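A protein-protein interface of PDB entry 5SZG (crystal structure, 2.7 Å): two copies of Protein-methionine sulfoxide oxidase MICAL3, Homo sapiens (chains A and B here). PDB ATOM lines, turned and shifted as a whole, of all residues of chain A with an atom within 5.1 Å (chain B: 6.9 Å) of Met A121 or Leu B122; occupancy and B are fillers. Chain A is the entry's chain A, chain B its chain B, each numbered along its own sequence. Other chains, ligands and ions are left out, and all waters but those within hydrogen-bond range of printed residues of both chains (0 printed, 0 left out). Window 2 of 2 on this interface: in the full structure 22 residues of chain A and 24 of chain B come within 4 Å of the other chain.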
ATOM      1  N   GLN A  88       2.085 -15.247   5.584  1.00  0.00           N
ATOM      2  CA  GLN A  88       1.138 -14.847   4.529  1.00  0.00           C
ATOM      3  C   GLN A  88       0.663 -16.054   3.720  1.00  0.00           C
ATOM      4  O   GLN A  88      -0.498 -16.190   3.433  1.00  0.00           O
ATOM      5  CB  GLN A  88       1.787 -13.801   3.624  1.00  0.00           C
ATOM      6  CG  GLN A  88       0.893 -13.278   2.478  1.00  0.00           C
ATOM      7  CD  GLN A  88       1.005 -14.030   1.142  1.00  0.00           C
ATOM      8  OE1 GLN A  88       0.030 -14.031   0.390  1.00  0.00           O
ATOM      9  NE2 GLN A  88       2.164 -14.671   0.820  1.00  0.00           N
ATOM     10  N   LEU A  91      -1.852 -18.108   5.718  1.00  0.00           N
ATOM     11  CA  LEU A  91      -3.143 -17.414   5.789  1.00  0.00           C
ATOM     12  C   LEU A  91      -3.874 -17.497   4.475  1.00  0.00           C
ATOM     13  O   LEU A  91      -5.110 -17.513   4.425  1.00  0.00           O
ATOM     14  CB  LEU A  91      -2.946 -15.932   6.194  1.00  0.00           C
ATOM     15  CG  LEU A  91      -2.552 -15.694   7.679  1.00  0.00           C
ATOM     16  CD1 LEU A  91      -2.043 -14.270   7.942  1.00  0.00           C
ATOM     17  CD2 LEU A  91      -3.730 -15.988   8.584  1.00  0.00           C
ATOM     18  N   GLN A  92      -3.104 -17.449   3.405  1.00  0.00           N
ATOM     19  CA  GLN A  92      -3.662 -17.517   2.062  1.00  0.00           C
ATOM     20  C   GLN A  92      -4.211 -18.926   1.839  1.00  0.00           C
ATOM     21  O   GLN A  92      -5.247 -19.067   1.227  1.00  0.00           O
ATOM     22  CB  GLN A  92      -2.595 -17.176   1.056  1.00  0.00           C
ATOM     23  CG  GLN A  92      -3.103 -16.999  -0.366  1.00  0.00           C
ATOM     24  CD  GLN A  92      -1.993 -16.663  -1.357  1.00  0.00           C
ATOM     25  OE1 GLN A  92      -1.009 -15.974  -1.027  1.00  0.00           O
ATOM     26  NE2 GLN A  92      -2.148 -17.143  -2.592  1.00  0.00           N
ATOM     27  N   LEU A  95      -7.501 -19.162   3.743  1.00  0.00           N
ATOM     28  CA  LEU A  95      -8.507 -18.466   2.963  1.00  0.00           C
ATOM     29  C   LEU A  95      -8.959 -19.198   1.687  1.00  0.00           C
ATOM     30  O   LEU A  95     -10.148 -19.206   1.396  1.00  0.00           O
ATOM     31  CB  LEU A  95      -7.947 -17.106   2.594  1.00  0.00           C
ATOM     32  CG  LEU A  95      -8.872 -16.078   2.037  1.00  0.00           C
ATOM     33  CD1 LEU A  95      -9.853 -15.586   3.090  1.00  0.00           C
ATOM     34  CD2 LEU A  95      -8.046 -14.945   1.413  1.00  0.00           C
ATOM     35  N   ILE A 117      -9.466 -13.301   8.664  1.00  0.00           N
ATOM     36  CA  ILE A 117      -8.265 -13.922   8.078  1.00  0.00           C
ATOM     37  C   ILE A 117      -7.705 -12.925   7.078  1.00  0.00           C
ATOM     38  O   ILE A 117      -6.505 -12.713   7.016  1.00  0.00           O
ATOM     39  CB  ILE A 117      -8.574 -15.270   7.350  1.00  0.00           C
ATOM     40  CG1 ILE A 117      -8.758 -16.383   8.363  1.00  0.00           C
ATOM     41  CG2 ILE A 117      -7.463 -15.653   6.361  1.00  0.00           C
ATOM     42  CD1 ILE A 117      -9.616 -17.519   7.853  1.00  0.00           C
ATOM     43  N   LEU A 118      -8.589 -12.380   6.262  1.00  0.00           N
ATOM     44  CA  LEU A 118      -8.183 -11.414   5.265  1.00  0.00           C
ATOM     45  C   LEU A 118      -7.536 -10.171   5.895  1.00  0.00           C
ATOM     46  O   LEU A 118      -6.520  -9.788   5.412  1.00  0.00           O
ATOM     47  CB  LEU A 118      -9.352 -11.035   4.384  1.00  0.00           C
ATOM     48  CG  LEU A 118      -8.991 -10.196   3.188  1.00  0.00           C
ATOM     49  CD1 LEU A 118      -7.803 -10.717   2.396  1.00  0.00           C
ATOM     50  CD2 LEU A 118     -10.238 -10.068   2.284  1.00  0.00           C
ATOM     51  N   ASN A 119      -8.061  -9.632   7.014  1.00  0.00           N
ATOM     52  CA  ASN A 119      -7.374  -8.579   7.777  1.00  0.00           C
ATOM     53  C   ASN A 119      -6.011  -8.957   8.319  1.00  0.00           C
ATOM     54  O   ASN A 119      -5.103  -8.125   8.306  1.00  0.00           O
ATOM     55  CB  ASN A 119      -8.192  -8.046   8.975  1.00  0.00           C
ATOM     56  CG  ASN A 119      -9.505  -7.394   8.566  1.00  0.00           C
ATOM     57  OD1 ASN A 119      -9.713  -6.964   7.412  1.00  0.00           O
ATOM     58  ND2 ASN A 119     -10.437  -7.373   9.515  1.00  0.00           N
ATOM     59  N   GLU A 120      -5.862 -10.170   8.839  1.00  0.00           N
ATOM     60  CA  GLU A 120      -4.558 -10.630   9.328  1.00  0.00           C
ATOM     61  C   GLU A 120      -3.536 -10.576   8.184  1.00  0.00           C
ATOM     62  O   GLU A 120      -2.425 -10.050   8.331  1.00  0.00           O
ATOM     63  CB  GLU A 120      -4.632 -12.034   9.989  1.00  0.00           C
ATOM     64  CG  GLU A 120      -4.856 -11.993  11.495  1.00  0.00           C
ATOM     65  CD  GLU A 120      -5.052 -13.385  12.109  1.00  0.00           C
ATOM     66  OE1 GLU A 120      -4.109 -14.226  12.051  1.00  0.00           O
ATOM     67  OE2 GLU A 120      -6.162 -13.649  12.645  1.00  0.00           O
ATOM     68  N   MET A 121      -3.948 -11.096   7.040  1.00  0.00           N
ATOM     69  CA  MET A 121      -3.130 -11.134   5.826  1.00  0.00           C
ATOM     70  C   MET A 121      -2.778  -9.766   5.302  1.00  0.00           C
ATOM     71  O   MET A 121      -1.650  -9.583   4.844  1.00  0.00           O
ATOM     72  CB  MET A 121      -3.753 -11.958   4.771  1.00  0.00           C
ATOM     73  CG  MET A 121      -2.777 -12.262   3.656  1.00  0.00           C
ATOM     74  SD  MET A 121      -3.853 -13.139   2.267  1.00  0.00           S
ATOM     75  CE  MET A 121      -5.203 -14.181   3.273  1.00  0.00           C
ATOM     76  N   LEU A 122      -3.673  -8.785   5.432  1.00  0.00           N
ATOM     77  CA  LEU A 122      -3.346  -7.440   4.994  1.00  0.00           C
ATOM     78  C   LEU A 122      -2.361  -6.743   5.930  1.00  0.00           C
ATOM     79  O   LEU A 122      -1.567  -5.946   5.460  1.00  0.00           O
ATOM     80  CB  LEU A 122      -4.608  -6.622   4.755  1.00  0.00           C
ATOM     81  CG  LEU A 122      -5.474  -7.183   3.601  1.00  0.00           C
ATOM     82  CD1 LEU A 122      -6.735  -6.328   3.436  1.00  0.00           C
ATOM     83  CD2 LEU A 122      -4.727  -7.261   2.279  1.00  0.00           C
ATOM     84  N   GLU A 123      -2.409  -7.008   7.232  1.00  0.00           N
ATOM     85  CA  GLU A 123      -1.450  -6.392   8.102  1.00  0.00           C
ATOM     86  C   GLU A 123      -0.077  -7.080   8.095  1.00  0.00           C
ATOM     87  O   GLU A 123       0.913  -6.439   8.321  1.00  0.00           O
ATOM     88  CB  GLU A 123      -2.013  -6.054   9.469  1.00  0.00           C
ATOM     89  CG  GLU A 123      -1.983  -7.055  10.579  1.00  0.00           C
ATOM     90  CD  GLU A 123      -2.802  -6.569  11.788  1.00  0.00           C
ATOM     91  OE1 GLU A 123      -2.389  -6.852  12.934  1.00  0.00           O
ATOM     92  OE2 GLU A 123      -3.869  -5.913  11.605  1.00  0.00           O
ATOM     93  N   VAL A 124      -0.026  -8.346   7.726  1.00  0.00           N
ATOM     94  CA  VAL A 124       1.215  -9.017   7.364  1.00  0.00           C
ATOM     95  C   VAL A 124       1.830  -8.421   6.128  1.00  0.00           C
ATOM     96  O   VAL A 124       3.035  -8.179   6.084  1.00  0.00           O
ATOM     97  CB  VAL A 124       0.996 -10.533   7.130  1.00  0.00           C
ATOM     98  CG1 VAL A 124       2.148 -11.176   6.347  1.00  0.00           C
ATOM     99  CG2 VAL A 124       0.832 -11.232   8.477  1.00  0.00           C
ATOM    100  N   VAL A 125       1.020  -8.164   5.123  1.00  0.00           N
ATOM    101  CA  VAL A 125       1.501  -7.503   3.932  1.00  0.00           C
ATOM    102  C   VAL A 125       1.998  -6.089   4.259  1.00  0.00           C
ATOM    103  O   VAL A 125       2.952  -5.659   3.676  1.00  0.00           O
ATOM    104  CB  VAL A 125       0.447  -7.521   2.808  1.00  0.00           C
ATOM    105  CG1 VAL A 125       0.725  -6.506   1.710  1.00  0.00           C
ATOM    106  CG2 VAL A 125       0.384  -8.901   2.179  1.00  0.00           C
ATOM    107  N   LEU B  91      -5.714  -1.733  -5.220  1.00  0.00           N
ATOM    108  CA  LEU B  91      -6.598  -2.887  -5.254  1.00  0.00           C
ATOM    109  C   LEU B  91      -7.176  -3.165  -3.865  1.00  0.00           C
ATOM    110  O   LEU B  91      -8.317  -3.568  -3.731  1.00  0.00           O
ATOM    111  CB  LEU B  91      -5.838  -4.129  -5.715  1.00  0.00           C
ATOM    112  CG  LEU B  91      -5.493  -4.207  -7.212  1.00  0.00           C
ATOM    113  CD1 LEU B  91      -4.485  -5.322  -7.535  1.00  0.00           C
ATOM    114  CD2 LEU B  91      -6.750  -4.392  -8.050  1.00  0.00           C
ATOM    115  N   ILE B 117     -10.853  -9.092  -7.761  1.00  0.00           N
ATOM    116  CA  ILE B 117      -9.974  -8.072  -7.236  1.00  0.00           C
ATOM    117  C   ILE B 117      -9.038  -8.720  -6.245  1.00  0.00           C
ATOM    118  O   ILE B 117      -7.839  -8.477  -6.265  1.00  0.00           O
ATOM    119  CB  ILE B 117     -10.755  -6.936  -6.523  1.00  0.00           C
ATOM    120  CG1 ILE B 117     -11.387  -5.980  -7.547  1.00  0.00           C
ATOM    121  CG2 ILE B 117      -9.865  -6.141  -5.582  1.00  0.00           C
ATOM    122  CD1 ILE B 117     -12.594  -5.229  -7.005  1.00  0.00           C
ATOM    123  N   LEU B 118      -9.595  -9.550  -5.382  1.00  0.00           N
ATOM    124  CA  LEU B 118      -8.794 -10.256  -4.444  1.00  0.00           C
ATOM    125  C   LEU B 118      -7.741 -11.088  -5.133  1.00  0.00           C
ATOM    126  O   LEU B 118      -6.596 -11.119  -4.658  1.00  0.00           O
ATOM    127  CB  LEU B 118      -9.661 -11.110  -3.516  1.00  0.00           C
ATOM    128  CG  LEU B 118      -8.940 -11.844  -2.375  1.00  0.00           C
ATOM    129  CD1 LEU B 118      -8.131 -10.910  -1.498  1.00  0.00           C
ATOM    130  CD2 LEU B 118      -9.947 -12.654  -1.558  1.00  0.00           C
ATOM    131  N   ASN B 119      -8.090 -11.792  -6.206  1.00  0.00           N
ATOM    132  CA  ASN B 119      -7.071 -12.588  -6.950  1.00  0.00           C
ATOM    133  C   ASN B 119      -5.983 -11.750  -7.602  1.00  0.00           C
ATOM    134  O   ASN B 119      -4.832 -12.161  -7.618  1.00  0.00           O
ATOM    135  CB  ASN B 119      -7.699 -13.481  -8.029  1.00  0.00           C
ATOM    136  CG  ASN B 119      -8.415 -14.710  -7.455  1.00  0.00           C
ATOM    137  OD1 ASN B 119      -8.589 -14.874  -6.234  1.00  0.00           O
ATOM    138  ND2 ASN B 119      -8.823 -15.604  -8.355  1.00  0.00           N
ATOM    139  N   GLU B 120      -6.342 -10.614  -8.176  1.00  0.00           N
ATOM    140  CA  GLU B 120      -5.331  -9.715  -8.750  1.00  0.00           C
ATOM    141  C   GLU B 120      -4.336  -9.314  -7.666  1.00  0.00           C
ATOM    142  O   GLU B 120      -3.140  -9.373  -7.848  1.00  0.00           O
ATOM    143  CB  GLU B 120      -5.977  -8.495  -9.416  1.00  0.00           C
ATOM    144  N   MET B 121      -4.855  -8.982  -6.498  1.00  0.00           N
ATOM    145  CA  MET B 121      -4.004  -8.617  -5.357  1.00  0.00           C
ATOM    146  C   MET B 121      -3.087  -9.687  -4.838  1.00  0.00           C
ATOM    147  O   MET B 121      -2.002  -9.387  -4.381  1.00  0.00           O
ATOM    148  CB  MET B 121      -4.954  -8.307  -4.267  1.00  0.00           C
ATOM    149  CG  MET B 121      -4.564  -7.016  -3.618  1.00  0.00           C
ATOM    150  SD  MET B 121      -5.746  -6.942  -2.033  1.00  0.00           S
ATOM    151  CE  MET B 121      -4.146  -7.124  -0.886  1.00  0.00           C
ATOM    152  N   LEU B 122      -3.532 -10.945  -4.866  1.00  0.00           N
ATOM    153  CA  LEU B 122      -2.699 -12.056  -4.422  1.00  0.00           C
ATOM    154  C   LEU B 122      -1.596 -12.386  -5.413  1.00  0.00           C
ATOM    155  O   LEU B 122      -0.496 -12.738  -4.978  1.00  0.00           O
ATOM    156  CB  LEU B 122      -3.530 -13.277  -4.077  1.00  0.00           C
ATOM    157  CG  LEU B 122      -4.461 -13.086  -2.887  1.00  0.00           C
ATOM    158  CD1 LEU B 122      -5.284 -14.346  -2.649  1.00  0.00           C
ATOM    159  CD2 LEU B 122      -3.728 -12.683  -1.621  1.00  0.00           C
ATOM    160  N   GLU B 123      -1.850 -12.172  -6.710  1.00  0.00           N
ATOM    161  CA  GLU B 123      -0.809 -12.251  -7.740  1.00  0.00           C
ATOM    162  C   GLU B 123       0.232 -11.124  -7.641  1.00  0.00           C
ATOM    163  O   GLU B 123       1.392 -11.315  -7.947  1.00  0.00           O
ATOM    164  CB  GLU B 123      -1.437 -12.271  -9.147  1.00  0.00           C
ATOM    165  CG  GLU B 123      -2.284 -13.540  -9.424  1.00  0.00           C
ATOM    166  CD  GLU B 123      -1.738 -14.466 -10.535  1.00  0.00           C
ATOM    167  OE1 GLU B 123      -0.511 -14.417 -10.816  1.00  0.00           O
ATOM    168  OE2 GLU B 123      -2.535 -15.263 -11.123  1.00  0.00           O
ATOM    169  N   VAL B 124      -0.206  -9.941  -7.282  1.00  0.00           N
ATOM    170  CA  VAL B 124       0.678  -8.809  -7.048  1.00  0.00           C
ATOM    171  C   VAL B 124       1.554  -9.063  -5.857  1.00  0.00           C
ATOM    172  O   VAL B 124       2.768  -8.767  -5.912  1.00  0.00           O
ATOM    173  CB  VAL B 124      -0.118  -7.514  -6.844  1.00  0.00           C
ATOM    174  CG1 VAL B 124       0.750  -6.418  -6.192  1.00  0.00           C
ATOM    175  CG2 VAL B 124      -0.662  -7.028  -8.182  1.00  0.00           C
ATOM    176  N   VAL B 125       0.962  -9.597  -4.784  1.00  0.00           N
ATOM    177  CA  VAL B 125       1.764 -10.020  -3.611  1.00  0.00           C
ATOM    178  C   VAL B 125       2.794 -11.095  -3.959  1.00  0.00           C
ATOM    179  O   VAL B 125       3.930 -11.022  -3.501  1.00  0.00           O
ATOM    180  CB  VAL B 125       0.886 -10.444  -2.413  1.00  0.00           C
ATOM    181  CG1 VAL B 125       1.658 -11.231  -1.357  1.00  0.00           C
ATOM    182  CG2 VAL B 125       0.282  -9.211  -1.773  1.00  0.00           C
ATOM    183  N   GLU B 126       2.441 -12.037  -4.817  1.00  0.00           N
ATOM    184  CA  GLU B 126       3.385 -13.095  -5.205  1.00  0.00           C
ATOM    185  C   GLU B 126       4.573 -12.541  -6.036  1.00  0.00           C
ATOM    186  O   GLU B 126       5.725 -12.882  -5.796  1.00  0.00           O
ATOM    187  CB  GLU B 126       2.665 -14.212  -5.944  1.00  0.00           C
ATOM    188  CG  GLU B 126       3.378 -15.550  -5.992  1.00  0.00           C
ATOM    189  CD  GLU B 126       2.948 -16.365  -7.213  1.00  0.00           C
ATOM    190  OE1 GLU B 126       2.141 -17.309  -7.031  1.00  0.00           O
ATOM    191  OE2 GLU B 126       3.379 -16.038  -8.358  1.00  0.00           O
ATOM    192  N   GLN B 127       4.285 -11.661  -6.984  1.00  0.00           N
ATOM    193  CA  GLN B 127       5.333 -10.998  -7.756  1.00  0.00           C
ATOM    194  C   GLN B 127       6.309 -10.198  -6.867  1.00  0.00           C
ATOM    195  O   GLN B 127       7.491 -10.202  -7.123  1.00  0.00           O
ATOM    196  CB  GLN B 127       4.735 -10.078  -8.811  1.00  0.00           C
ATOM    197  CG  GLN B 127       4.107 -10.775 -10.003  1.00  0.00           C
ATOM    198  CD  GLN B 127       3.523  -9.767 -11.006  1.00  0.00           C
ATOM    199  OE1 GLN B 127       4.146  -8.731 -11.310  1.00  0.00           O
ATOM    200  NE2 GLN B 127       2.327 -10.068 -11.526  1.00  0.00           N
ATOM    201  N   ASP B 129       7.032 -10.852  -3.633  1.00  0.00           N
ATOM    202  CA  ASP B 129       7.828 -11.937  -2.963  1.00  0.00           C
ATOM    203  C   ASP B 129       8.997 -12.336  -3.882  1.00  0.00           C
ATOM    204  O   ASP B 129      10.145 -12.575  -3.476  1.00  0.00           O
ATOM    205  CB  ASP B 129       7.005 -13.244  -2.793  1.00  0.00           C
ATOM    206  CG  ASP B 129       5.769 -13.159  -1.809  1.00  0.00           C
ATOM    207  OD1 ASP B 129       5.653 -12.260  -0.942  1.00  0.00           O
ATOM    208  OD2 ASP B 129       4.887 -14.058  -1.908  1.00  0.00           O
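Leu A118 touches its own counterpart, Leu B118.
Met A121 touches Leu B122, and with the chains exchanged Leu A122 touches Met B121.
Val B125 touches its own counterpart, Val A125.
The side-chain amide oxygen (OE1) of Gln A88 lies close to the side-chain amide oxygen (OE1) of Gln A92, at 2.6 Å.
Among the printed residues, pairs that only touch across the chains: Leu A122 with Met B121, Gln A88 with Val B125, Gln A88 with Asp B129, Leu A118 with Leu B118, Met A121 with Leu B122 and Val A125 with Val B125.
Of the printed residues of chain B, Gln A88 touches Val B125 (3.7 Å) and Asp B129 (3.9 Å).
Met A121 touches just one residue of chain B: Leu B122.
Printed residues of chain A within 4 Å of Met B121: Leu A122.
Of chain A, only Met A121 comes within 4 Å of Leu B122.
Of the printed residues of chain A, Val B125 touches Gln A88 and Val A125.
The nearest residue of chain B that does not touch Met A121 is Leu B118 (6.1 Å).
Printed residues of chain B that touch a printed residue of chain A: Leu B118, Met B121, Leu B122, Val B125 and Asp B129.
Hydrophobic or aromatic side chains of chain B within 4 Å of the printed part of chain A: Leu B118, Met B121, Leu B122 and Val B125.
Of the 13 printed residues of chain A, 5 touch a printed residue of chain B.
Hydrophobic or aromatic side chains of chain A that line the printed part of chain B: Leu A118, Met A121, Leu A122 and Val A125.
Among the printed residues, no Asp or Glu carboxylate lies within 4 Å of a Lys or Arg side-chain nitrogen of the other chain.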
